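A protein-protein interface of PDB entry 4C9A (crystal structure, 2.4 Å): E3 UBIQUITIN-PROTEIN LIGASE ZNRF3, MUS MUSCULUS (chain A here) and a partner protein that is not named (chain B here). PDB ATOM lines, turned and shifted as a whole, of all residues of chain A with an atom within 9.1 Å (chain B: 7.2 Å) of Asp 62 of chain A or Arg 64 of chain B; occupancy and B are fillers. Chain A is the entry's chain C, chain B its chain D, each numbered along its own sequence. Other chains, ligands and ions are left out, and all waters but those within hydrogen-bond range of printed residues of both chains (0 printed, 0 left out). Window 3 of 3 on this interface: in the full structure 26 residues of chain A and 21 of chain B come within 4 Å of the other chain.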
ATOM      1  N   MET A  49       4.493 -19.252  -6.292  1.00  0.00           N
ATOM      2  CA  MET A  49       5.093 -19.518  -7.577  1.00  0.00           C
ATOM      3  C   MET A  49       5.722 -18.243  -8.172  1.00  0.00           C
ATOM      4  O   MET A  49       5.172 -17.156  -8.128  1.00  0.00           O
ATOM      5  CB  MET A  49       4.103 -20.135  -8.522  1.00  0.00           C
ATOM      6  CG  MET A  49       3.504 -21.420  -8.055  1.00  0.00           C
ATOM      7  SD  MET A  49       4.449 -22.929  -8.150  1.00  0.00           S
ATOM      8  CE  MET A  49       4.796 -22.829  -9.897  1.00  0.00           C
ATOM      9  N   GLY A  53       7.652 -19.128 -13.060  1.00  0.00           N
ATOM     10  CA  GLY A  53       7.600 -20.500 -12.542  1.00  0.00           C
ATOM     11  C   GLY A  53       6.494 -21.301 -13.174  1.00  0.00           C
ATOM     12  O   GLY A  53       6.365 -22.499 -12.905  1.00  0.00           O
ATOM     13  N   ASN A  58       7.710 -26.781 -20.704  1.00  0.00           N
ATOM     14  CA  ASN A  58       8.448 -27.859 -20.049  1.00  0.00           C
ATOM     15  C   ASN A  58       7.669 -29.143 -20.236  1.00  0.00           C
ATOM     16  O   ASN A  58       6.456 -29.174 -20.019  1.00  0.00           O
ATOM     17  CB  ASN A  58       8.619 -27.599 -18.560  1.00  0.00           C
ATOM     18  CG  ASN A  58       9.589 -26.477 -18.271  1.00  0.00           C
ATOM     19  OD1 ASN A  58      10.652 -26.698 -17.695  1.00  0.00           O
ATOM     20  ND2 ASN A  58       9.231 -25.266 -18.674  1.00  0.00           N
ATOM     21  N   ASP A  59       8.357 -30.201 -20.639  1.00  0.00           N
ATOM     22  CA  ASP A  59       7.676 -31.452 -20.942  1.00  0.00           C
ATOM     23  C   ASP A  59       7.110 -32.064 -19.648  1.00  0.00           C
ATOM     24  O   ASP A  59       5.988 -32.574 -19.639  1.00  0.00           O
ATOM     25  CB  ASP A  59       8.620 -32.421 -21.669  1.00  0.00           C
ATOM     26  CG  ASP A  59       9.227 -31.812 -22.935  1.00  0.00           C
ATOM     27  OD1 ASP A  59       8.469 -31.345 -23.821  1.00  0.00           O
ATOM     28  OD2 ASP A  59      10.473 -31.808 -23.036  1.00  0.00           O
ATOM     29  N   GLU A  60       7.897 -31.991 -18.574  1.00  0.00           N
ATOM     30  CA  GLU A  60       7.503 -32.454 -17.248  1.00  0.00           C
ATOM     31  C   GLU A  60       7.967 -31.408 -16.281  1.00  0.00           C
ATOM     32  O   GLU A  60       9.134 -31.008 -16.308  1.00  0.00           O
ATOM     33  CB  GLU A  60       8.206 -33.759 -16.857  1.00  0.00           C
ATOM     34  CG  GLU A  60       8.266 -34.829 -17.934  1.00  0.00           C
ATOM     35  CD  GLU A  60       9.567 -35.607 -17.898  1.00  0.00           C
ATOM     36  OE1 GLU A  60      10.622 -35.002 -18.175  1.00  0.00           O
ATOM     37  OE2 GLU A  60       9.540 -36.819 -17.606  1.00  0.00           O
ATOM     38  N   GLU A  61       7.080 -30.967 -15.413  1.00  0.00           N
ATOM     39  CA  GLU A  61       7.507 -30.069 -14.377  1.00  0.00           C
ATOM     40  C   GLU A  61       7.579 -30.833 -13.052  1.00  0.00           C
ATOM     41  O   GLU A  61       7.021 -31.948 -12.925  1.00  0.00           O
ATOM     42  CB  GLU A  61       6.580 -28.852 -14.335  1.00  0.00           C
ATOM     43  CG  GLU A  61       7.128 -27.631 -15.090  1.00  0.00           C
ATOM     44  CD  GLU A  61       6.086 -26.874 -15.933  1.00  0.00           C
ATOM     45  OE1 GLU A  61       4.896 -27.267 -15.988  1.00  0.00           O
ATOM     46  OE2 GLU A  61       6.468 -25.870 -16.573  1.00  0.00           O
ATOM     47  N   ASP A  62       8.316 -30.249 -12.101  1.00  0.00           N
ATOM     48  CA  ASP A  62       8.339 -30.724 -10.698  1.00  0.00           C
ATOM     49  C   ASP A  62       6.914 -30.833 -10.127  1.00  0.00           C
ATOM     50  O   ASP A  62       5.984 -30.098 -10.545  1.00  0.00           O
ATOM     51  CB  ASP A  62       9.147 -29.776  -9.798  1.00  0.00           C
ATOM     52  CG  ASP A  62      10.612 -29.673 -10.207  1.00  0.00           C
ATOM     53  OD1 ASP A  62      11.296 -30.711 -10.369  1.00  0.00           O
ATOM     54  OD2 ASP A  62      11.090 -28.533 -10.359  1.00  0.00           O
ATOM     55  N   LEU A  63       6.721 -31.739  -9.176  1.00  0.00           N
ATOM     56  CA  LEU A  63       5.337 -32.042  -8.784  1.00  0.00           C
ATOM     57  C   LEU A  63       4.992 -31.606  -7.371  1.00  0.00           C
ATOM     58  O   LEU A  63       5.723 -31.913  -6.438  1.00  0.00           O
ATOM     59  CB  LEU A  63       5.027 -33.527  -8.983  1.00  0.00           C
ATOM     60  CG  LEU A  63       3.550 -33.871  -9.199  1.00  0.00           C
ATOM     61  CD1 LEU A  63       2.849 -32.910 -10.159  1.00  0.00           C
ATOM     62  CD2 LEU A  63       3.441 -35.306  -9.715  1.00  0.00           C
ATOM     63  N   TYR A  64       3.891 -30.866  -7.242  1.00  0.00           N
ATOM     64  CA  TYR A  64       3.354 -30.477  -5.927  1.00  0.00           C
ATOM     65  C   TYR A  64       2.125 -31.327  -5.580  1.00  0.00           C
ATOM     66  O   TYR A  64       1.381 -31.775  -6.453  1.00  0.00           O
ATOM     67  CB  TYR A  64       3.047 -28.959  -5.858  1.00  0.00           C
ATOM     68  CG  TYR A  64       4.245 -28.097  -6.246  1.00  0.00           C
ATOM     69  CD1 TYR A  64       5.235 -27.790  -5.313  1.00  0.00           C
ATOM     70  CD2 TYR A  64       4.412 -27.650  -7.569  1.00  0.00           C
ATOM     71  CE1 TYR A  64       6.349 -27.051  -5.690  1.00  0.00           C
ATOM     72  CE2 TYR A  64       5.513 -26.903  -7.959  1.00  0.00           C
ATOM     73  CZ  TYR A  64       6.491 -26.605  -7.026  1.00  0.00           C
ATOM     74  OH  TYR A  64       7.613 -25.864  -7.382  1.00  0.00           O
ATOM     75  N   GLU A  65       1.947 -31.577  -4.287  1.00  0.00           N
ATOM     76  CA  GLU A  65       0.869 -32.428  -3.807  1.00  0.00           C
ATOM     77  C   GLU A  65      -0.433 -31.745  -4.178  1.00  0.00           C
ATOM     78  O   GLU A  65      -0.550 -30.544  -3.976  1.00  0.00           O
ATOM     79  CB  GLU A  65       0.965 -32.641  -2.291  1.00  0.00           C
ATOM     80  CG  GLU A  65       2.335 -33.099  -1.765  1.00  0.00           C
ATOM     81  CD  GLU A  65       3.303 -31.941  -1.394  1.00  0.00           C
ATOM     82  OE1 GLU A  65       3.621 -31.048  -2.258  1.00  0.00           O
ATOM     83  OE2 GLU A  65       3.774 -31.933  -0.219  1.00  0.00           O
ATOM     84  N   TRP A  68      -3.017 -27.359  -3.336  1.00  0.00           N
ATOM     85  CA  TRP A  68      -2.289 -26.203  -2.913  1.00  0.00           C
ATOM     86  C   TRP A  68      -2.893 -24.901  -3.367  1.00  0.00           C
ATOM     87  O   TRP A  68      -3.517 -24.822  -4.407  1.00  0.00           O
ATOM     88  CB  TRP A  68      -0.803 -26.251  -3.372  1.00  0.00           C
ATOM     89  CG  TRP A  68      -0.504 -26.541  -4.784  1.00  0.00           C
ATOM     90  CD1 TRP A  68      -0.409 -27.766  -5.334  1.00  0.00           C
ATOM     91  CD2 TRP A  68      -0.190 -25.610  -5.832  1.00  0.00           C
ATOM     92  NE1 TRP A  68      -0.124 -27.673  -6.679  1.00  0.00           N
ATOM     93  CE2 TRP A  68       0.051 -26.360  -7.002  1.00  0.00           C
ATOM     94  CE3 TRP A  68      -0.082 -24.225  -5.899  1.00  0.00           C
ATOM     95  CZ2 TRP A  68       0.391 -25.770  -8.227  1.00  0.00           C
ATOM     96  CZ3 TRP A  68       0.251 -23.640  -7.128  1.00  0.00           C
ATOM     97  CH2 TRP A  68       0.491 -24.417  -8.268  1.00  0.00           C
ATOM     98  N   ARG A  93      -2.672 -22.847 -15.822  1.00  0.00           N
ATOM     99  CA  ARG A  93      -1.551 -23.727 -15.652  1.00  0.00           C
ATOM    100  C   ARG A  93      -1.374 -24.160 -14.179  1.00  0.00           C
ATOM    101  O   ARG A  93      -0.928 -25.277 -13.891  1.00  0.00           O
ATOM    102  CB  ARG A  93      -0.339 -22.964 -16.164  1.00  0.00           C
ATOM    103  CG  ARG A  93       0.941 -23.733 -16.212  1.00  0.00           C
ATOM    104  CD  ARG A  93       1.255 -24.196 -17.621  1.00  0.00           C
ATOM    105  NE  ARG A  93       2.012 -25.433 -17.478  1.00  0.00           N
ATOM    106  CZ  ARG A  93       1.457 -26.632 -17.360  1.00  0.00           C
ATOM    107  NH1 ARG A  93       0.125 -26.773 -17.409  1.00  0.00           N
ATOM    108  NH2 ARG A  93       2.237 -27.699 -17.196  1.00  0.00           N
ATOM    109  N   ARG A  97      -1.847 -27.943 -12.587  1.00  0.00           N
ATOM    110  CA  ARG A  97      -0.843 -28.611 -11.739  1.00  0.00           C
ATOM    111  C   ARG A  97      -1.318 -28.737 -10.302  1.00  0.00           C
ATOM    112  O   ARG A  97      -0.548 -29.040  -9.409  1.00  0.00           O
ATOM    113  CB  ARG A  97       0.469 -27.882 -11.804  1.00  0.00           C
ATOM    114  CG  ARG A  97       0.969 -27.771 -13.232  1.00  0.00           C
ATOM    115  CD  ARG A  97       2.079 -26.753 -13.375  1.00  0.00           C
ATOM    116  NE  ARG A  97       3.217 -27.091 -12.522  1.00  0.00           N
ATOM    117  CZ  ARG A  97       4.257 -26.300 -12.288  1.00  0.00           C
ATOM    118  NH1 ARG A  97       4.329 -25.100 -12.850  1.00  0.00           N
ATOM    119  NH2 ARG A  97       5.237 -26.726 -11.488  1.00  0.00           N
ATOM    120  N   GLY A  98      -2.610 -28.498 -10.099  1.00  0.00           N
ATOM    121  CA  GLY A  98      -3.325 -29.034  -8.936  1.00  0.00           C
ATOM    122  C   GLY A  98      -3.639 -27.982  -7.927  1.00  0.00           C
ATOM    123  O   GLY A  98      -4.013 -28.275  -6.802  1.00  0.00           O
ATOM    124  N   TYR B  31      17.631 -19.671 -12.492  1.00  0.00           N
ATOM    125  CA  TYR B  31      17.245 -20.845 -11.720  1.00  0.00           C
ATOM    126  C   TYR B  31      16.122 -20.500 -10.724  1.00  0.00           C
ATOM    127  O   TYR B  31      16.196 -19.479 -10.068  1.00  0.00           O
ATOM    128  CB  TYR B  31      18.457 -21.325 -10.943  1.00  0.00           C
ATOM    129  CG  TYR B  31      18.190 -22.461  -9.995  1.00  0.00           C
ATOM    130  CD1 TYR B  31      17.774 -23.682 -10.457  1.00  0.00           C
ATOM    131  CD2 TYR B  31      18.419 -22.322  -8.643  1.00  0.00           C
ATOM    132  CE1 TYR B  31      17.578 -24.748  -9.585  1.00  0.00           C
ATOM    133  CE2 TYR B  31      18.248 -23.373  -7.764  1.00  0.00           C
ATOM    134  CZ  TYR B  31      17.816 -24.589  -8.231  1.00  0.00           C
ATOM    135  OH  TYR B  31      17.597 -25.651  -7.348  1.00  0.00           O
ATOM    136  N   LEU B  32      15.081 -21.324 -10.641  1.00  0.00           N
ATOM    137  CA  LEU B  32      14.098 -21.202  -9.556  1.00  0.00           C
ATOM    138  C   LEU B  32      14.558 -21.925  -8.306  1.00  0.00           C
ATOM    139  O   LEU B  32      14.697 -23.126  -8.316  1.00  0.00           O
ATOM    140  CB  LEU B  32      12.762 -21.760  -9.985  1.00  0.00           C
ATOM    141  CG  LEU B  32      12.210 -21.007 -11.191  1.00  0.00           C
ATOM    142  CD1 LEU B  32      10.936 -21.668 -11.701  1.00  0.00           C
ATOM    143  CD2 LEU B  32      12.006 -19.520 -10.889  1.00  0.00           C
ATOM    144  N   GLN B  39       9.452 -19.379  -3.848  1.00  0.00           N
ATOM    145  CA  GLN B  39      10.077 -19.714  -5.143  1.00  0.00           C
ATOM    146  C   GLN B  39      10.567 -18.407  -5.688  1.00  0.00           C
ATOM    147  O   GLN B  39       9.749 -17.548  -6.046  1.00  0.00           O
ATOM    148  CB  GLN B  39       9.106 -20.335  -6.154  1.00  0.00           C
ATOM    149  CG  GLN B  39       9.809 -20.975  -7.375  1.00  0.00           C
ATOM    150  CD  GLN B  39       8.868 -21.418  -8.485  1.00  0.00           C
ATOM    151  OE1 GLN B  39       8.057 -20.645  -9.020  1.00  0.00           O
ATOM    152  NE2 GLN B  39       8.964 -22.669  -8.837  1.00  0.00           N
ATOM    153  N   PRO B  49      24.186 -28.798  -9.248  1.00  0.00           N
ATOM    154  CA  PRO B  49      24.202 -30.229  -9.510  1.00  0.00           C
ATOM    155  C   PRO B  49      22.775 -30.774  -9.590  1.00  0.00           C
ATOM    156  O   PRO B  49      21.888 -30.301  -8.867  1.00  0.00           O
ATOM    157  CB  PRO B  49      24.962 -30.797  -8.301  1.00  0.00           C
ATOM    158  CG  PRO B  49      25.689 -29.634  -7.678  1.00  0.00           C
ATOM    159  CD  PRO B  49      24.817 -28.449  -7.958  1.00  0.00           C
ATOM    160  N   GLY B  50      22.556 -31.737 -10.481  1.00  0.00           N
ATOM    161  CA  GLY B  50      21.217 -32.259 -10.743  1.00  0.00           C
ATOM    162  C   GLY B  50      20.511 -31.472 -11.834  1.00  0.00           C
ATOM    163  O   GLY B  50      19.394 -31.811 -12.266  1.00  0.00           O
ATOM    164  N   TYR B  51      21.168 -30.419 -12.306  1.00  0.00           N
ATOM    165  CA  TYR B  51      20.604 -29.593 -13.340  1.00  0.00           C
ATOM    166  C   TYR B  51      21.586 -29.360 -14.490  1.00  0.00           C
ATOM    167  O   TYR B  51      22.785 -29.575 -14.352  1.00  0.00           O
ATOM    168  CB  TYR B  51      20.242 -28.273 -12.720  1.00  0.00           C
ATOM    169  CG  TYR B  51      19.106 -28.335 -11.783  1.00  0.00           C
ATOM    170  CD1 TYR B  51      19.278 -28.759 -10.476  1.00  0.00           C
ATOM    171  CD2 TYR B  51      17.838 -27.947 -12.193  1.00  0.00           C
ATOM    172  CE1 TYR B  51      18.206 -28.802  -9.589  1.00  0.00           C
ATOM    173  CE2 TYR B  51      16.763 -27.978 -11.322  1.00  0.00           C
ATOM    174  CZ  TYR B  51      16.941 -28.409 -10.018  1.00  0.00           C
ATOM    175  OH  TYR B  51      15.847 -28.429  -9.165  1.00  0.00           O
ATOM    176  N   TYR B  52      21.046 -28.876 -15.604  1.00  0.00           N
ATOM    177  CA  TYR B  52      21.796 -28.549 -16.791  1.00  0.00           C
ATOM    178  C   TYR B  52      21.180 -27.334 -17.473  1.00  0.00           C
ATOM    179  O   TYR B  52      19.988 -27.003 -17.280  1.00  0.00           O
ATOM    180  CB  TYR B  52      21.745 -29.712 -17.747  1.00  0.00           C
ATOM    181  CG  TYR B  52      20.371 -29.939 -18.316  1.00  0.00           C
ATOM    182  CD1 TYR B  52      19.425 -30.687 -17.624  1.00  0.00           C
ATOM    183  CD2 TYR B  52      20.013 -29.389 -19.529  1.00  0.00           C
ATOM    184  CE1 TYR B  52      18.167 -30.900 -18.154  1.00  0.00           C
ATOM    185  CE2 TYR B  52      18.755 -29.582 -20.062  1.00  0.00           C
ATOM    186  CZ  TYR B  52      17.841 -30.341 -19.377  1.00  0.00           C
ATOM    187  OH  TYR B  52      16.609 -30.525 -19.914  1.00  0.00           O
ATOM    188  N   CYS B  62      17.998 -23.224 -16.125  1.00  0.00           N
ATOM    189  CA  CYS B  62      18.390 -24.521 -15.651  1.00  0.00           C
ATOM    190  C   CYS B  62      17.192 -25.438 -15.757  1.00  0.00           C
ATOM    191  O   CYS B  62      16.075 -24.979 -15.620  1.00  0.00           O
ATOM    192  CB  CYS B  62      18.892 -24.402 -14.220  1.00  0.00           C
ATOM    193  SG  CYS B  62      20.416 -23.443 -14.183  1.00  0.00           S
ATOM    194  N   SER B  63      17.425 -26.717 -16.040  1.00  0.00           N
ATOM    195  CA  SER B  63      16.369 -27.718 -16.040  1.00  0.00           C
ATOM    196  C   SER B  63      16.814 -28.918 -15.256  1.00  0.00           C
ATOM    197  O   SER B  63      18.033 -29.211 -15.164  1.00  0.00           O
ATOM    198  CB  SER B  63      16.019 -28.153 -17.447  1.00  0.00           C
ATOM    199  OG  SER B  63      15.550 -27.024 -18.145  1.00  0.00           O
ATOM    200  N   ARG B  64      15.822 -29.615 -14.689  1.00  0.00           N
ATOM    201  CA  ARG B  64      16.124 -30.776 -13.891  1.00  0.00           C
ATOM    202  C   ARG B  64      16.611 -31.875 -14.812  1.00  0.00           C
ATOM    203  O   ARG B  64      15.989 -32.187 -15.839  1.00  0.00           O
ATOM    204  CB  ARG B  64      14.944 -31.265 -13.039  1.00  0.00           C
ATOM    205  CG  ARG B  64      15.420 -32.226 -11.945  1.00  0.00           C
ATOM    206  CD  ARG B  64      14.315 -32.691 -11.023  1.00  0.00           C
ATOM    207  NE  ARG B  64      13.988 -31.668 -10.035  1.00  0.00           N
ATOM    208  CZ  ARG B  64      14.753 -31.342  -8.997  1.00  0.00           C
ATOM    209  NH1 ARG B  64      15.925 -31.949  -8.780  1.00  0.00           N
ATOM    210  NH2 ARG B  64      14.348 -30.388  -8.172  1.00  0.00           N
ATOM    211  N   CYS B  65      17.760 -32.416 -14.435  1.00  0.00           N
ATOM    212  CA  CYS B  65      18.328 -33.569 -15.075  1.00  0.00           C
ATOM    213  C   CYS B  65      17.397 -34.729 -14.732  1.00  0.00           C
ATOM    214  O   CYS B  65      17.266 -35.100 -13.553  1.00  0.00           O
ATOM    215  CB  CYS B  65      19.746 -33.786 -14.527  1.00  0.00           C
ATOM    216  SG  CYS B  65      20.708 -35.087 -15.312  1.00  0.00           S
ATOM    217  N   ARG B  66      16.710 -35.261 -15.747  1.00  0.00           N
ATOM    218  CA  ARG B  66      15.769 -36.382 -15.561  1.00  0.00           C
ATOM    219  C   ARG B  66      16.189 -37.644 -16.359  1.00  0.00           C
ATOM    220  O   ARG B  66      15.362 -38.318 -16.968  1.00  0.00           O
ATOM    221  CB  ARG B  66      14.332 -35.944 -15.902  1.00  0.00           C
ATOM    222  CG  ARG B  66      13.725 -34.891 -14.958  1.00  0.00           C
ATOM    223  CD  ARG B  66      12.195 -34.982 -14.911  1.00  0.00           C
ATOM    224  NE  ARG B  66      11.522 -33.675 -14.881  1.00  0.00           N
ATOM    225  CZ  ARG B  66      11.137 -33.026 -13.782  1.00  0.00           C
ATOM    226  NH1 ARG B  66      11.349 -33.533 -12.569  1.00  0.00           N
ATOM    227  NH2 ARG B  66      10.537 -31.847 -13.901  1.00  0.00           N
ATOM    228  N   ILE B  67      17.488 -37.941 -16.352  1.00  0.00           N
ATOM    229  CA  ILE B  67      18.017 -39.184 -16.914  1.00  0.00           C
ATOM    230  C   ILE B  67      17.961 -40.233 -15.805  1.00  0.00           C
ATOM    231  O   ILE B  67      18.660 -40.115 -14.777  1.00  0.00           O
ATOM    232  CB  ILE B  67      19.470 -39.021 -17.452  1.00  0.00           C
ATOM    233  CG1 ILE B  67      19.460 -38.272 -18.785  1.00  0.00           C
ATOM    234  CG2 ILE B  67      20.156 -40.370 -17.656  1.00  0.00           C
ATOM    235  CD1 ILE B  67      20.841 -37.900 -19.295  1.00  0.00           C
ATOM    236  N   CYS B  73      23.606 -34.216 -15.639  1.00  0.00           N
ATOM    237  CA  CYS B  73      23.460 -34.158 -17.092  1.00  0.00           C
ATOM    238  C   CYS B  73      24.419 -33.137 -17.636  1.00  0.00           C
ATOM    239  O   CYS B  73      24.621 -32.098 -17.013  1.00  0.00           O
ATOM    240  CB  CYS B  73      22.123 -33.542 -17.451  1.00  0.00           C
ATOM    241  SG  CYS B  73      20.706 -34.577 -17.286  1.00  0.00           S
ATOM    242  N   ARG B  76      19.914 -32.717 -21.676  1.00  0.00           N
ATOM    243  CA  ARG B  76      18.759 -33.529 -21.359  1.00  0.00           C
ATOM    244  C   ARG B  76      19.061 -35.014 -21.515  1.00  0.00           C
ATOM    245  O   ARG B  76      18.700 -35.805 -20.652  1.00  0.00           O
ATOM    246  CB  ARG B  76      17.569 -33.142 -22.232  1.00  0.00           C
ATOM    247  CG  ARG B  76      16.253 -33.743 -21.748  1.00  0.00           C
ATOM    248  CD  ARG B  76      15.251 -33.933 -22.878  1.00  0.00           C
ATOM    249  NE  ARG B  76      14.468 -32.721 -23.123  1.00  0.00           N
ATOM    250  CZ  ARG B  76      13.611 -32.562 -24.132  1.00  0.00           C
ATOM    251  NH1 ARG B  76      13.415 -33.530 -25.023  1.00  0.00           N
ATOM    252  NH2 ARG B  76      12.948 -31.423 -24.258  1.00  0.00           N
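The side-chain carboxylate (OD1) of Asp 62 of chain A lies within salt-bridge range of the guanidinium group (NH1) of Arg 66 of chain B.
OD2 of Asp 59 of chain A lies within salt-bridge range of NH2 of Arg 76 of chain B.
The side-chain carboxylate (OD1) of Asp 62 of chain A is in salt-bridge range of the guanidinium group (NE) of Arg 64 of chain B (2.9 Å).
NE of Arg 66 of chain B lies within salt-bridge range of OE1 of Glu 60 of chain A.
The side-chain hydroxyl (OH) of Tyr 51 of chain B is in hydrogen-bond range of the guanidinium group (NH2) of Arg 64 of chain B, at 2.7 Å.
The guanidinium group (NH1) of Arg 97 of chain A lies within hydrogen-bond range of the backbone carbonyl oxygen (O) of Gly 53 of chain A.
The side-chain carboxylate (OE1) of Glu 61 of chain A lies within salt-bridge range of the guanidinium group (NE) of Arg 97 of chain A, 3.9 Å away.
SG of Cys 73 of chain B is disulfide-bonded to SG of Cys 65 of chain B (2.0 Å).
The side-chain carboxylate (OE1) of Glu 61 of chain A is in salt-bridge range of the guanidinium group (NH2) of Arg 93 of chain A (3.0 Å).
Gln 39 of chain B touches Met 49 of chain A.
Gly 53 of chain A touches Leu 32 of chain B (CA to CD1, 3.6 Å).
OE1 of Gln 39 of chain B touches CA of Gly 53 of chain A, at 3.6 Å.
Arg 66 of chain B touches Glu 61 of chain A (NH2 to C, 3.2 Å).
Tyr 64 of chain A touches Gln 39 of chain B.
Asp 62 of chain A touches just these residues of chain B: Arg 64 (2.9 Å) and Arg 66 (3.3 Å).
Arg 64 of chain B touches just one residue of chain A: Asp 62.
No residue of chain A comes within 4 Å of Ser 63 of chain B.
Printed residues of chain B within 4 Å of Glu 61 of chain A: Arg 66 (3.2 Å).
Printed residues of chain B within 4 Å of Tyr 64 of chain A: Gln 39 (3.8 Å).
Printed residues of chain B within 4 Å of Glu 60 of chain A: Arg 66 (2.9 Å).
Of the printed residues of chain B, Gly 53 of chain A touches Leu 32 (3.6 Å) and Gln 39 (3.6 Å).
Cys 62 of chain B touches none of the printed residues of chain A.
The nearest residue of chain B that does not touch Asp 62 of chain A is Tyr 51 of chain B (4.9 Å).
The nearest printed residue of chain A that does not touch Gln 39 of chain B is Arg 97 of chain A (6.1 Å).
Printed residues of chain B that touch a printed residue of chain A: Leu 32, Gln 39, Arg 64, Arg 66 and Arg 76.
Hydrophobic or aromatic side chains of chain B that line the printed part of chain A: Leu 32.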
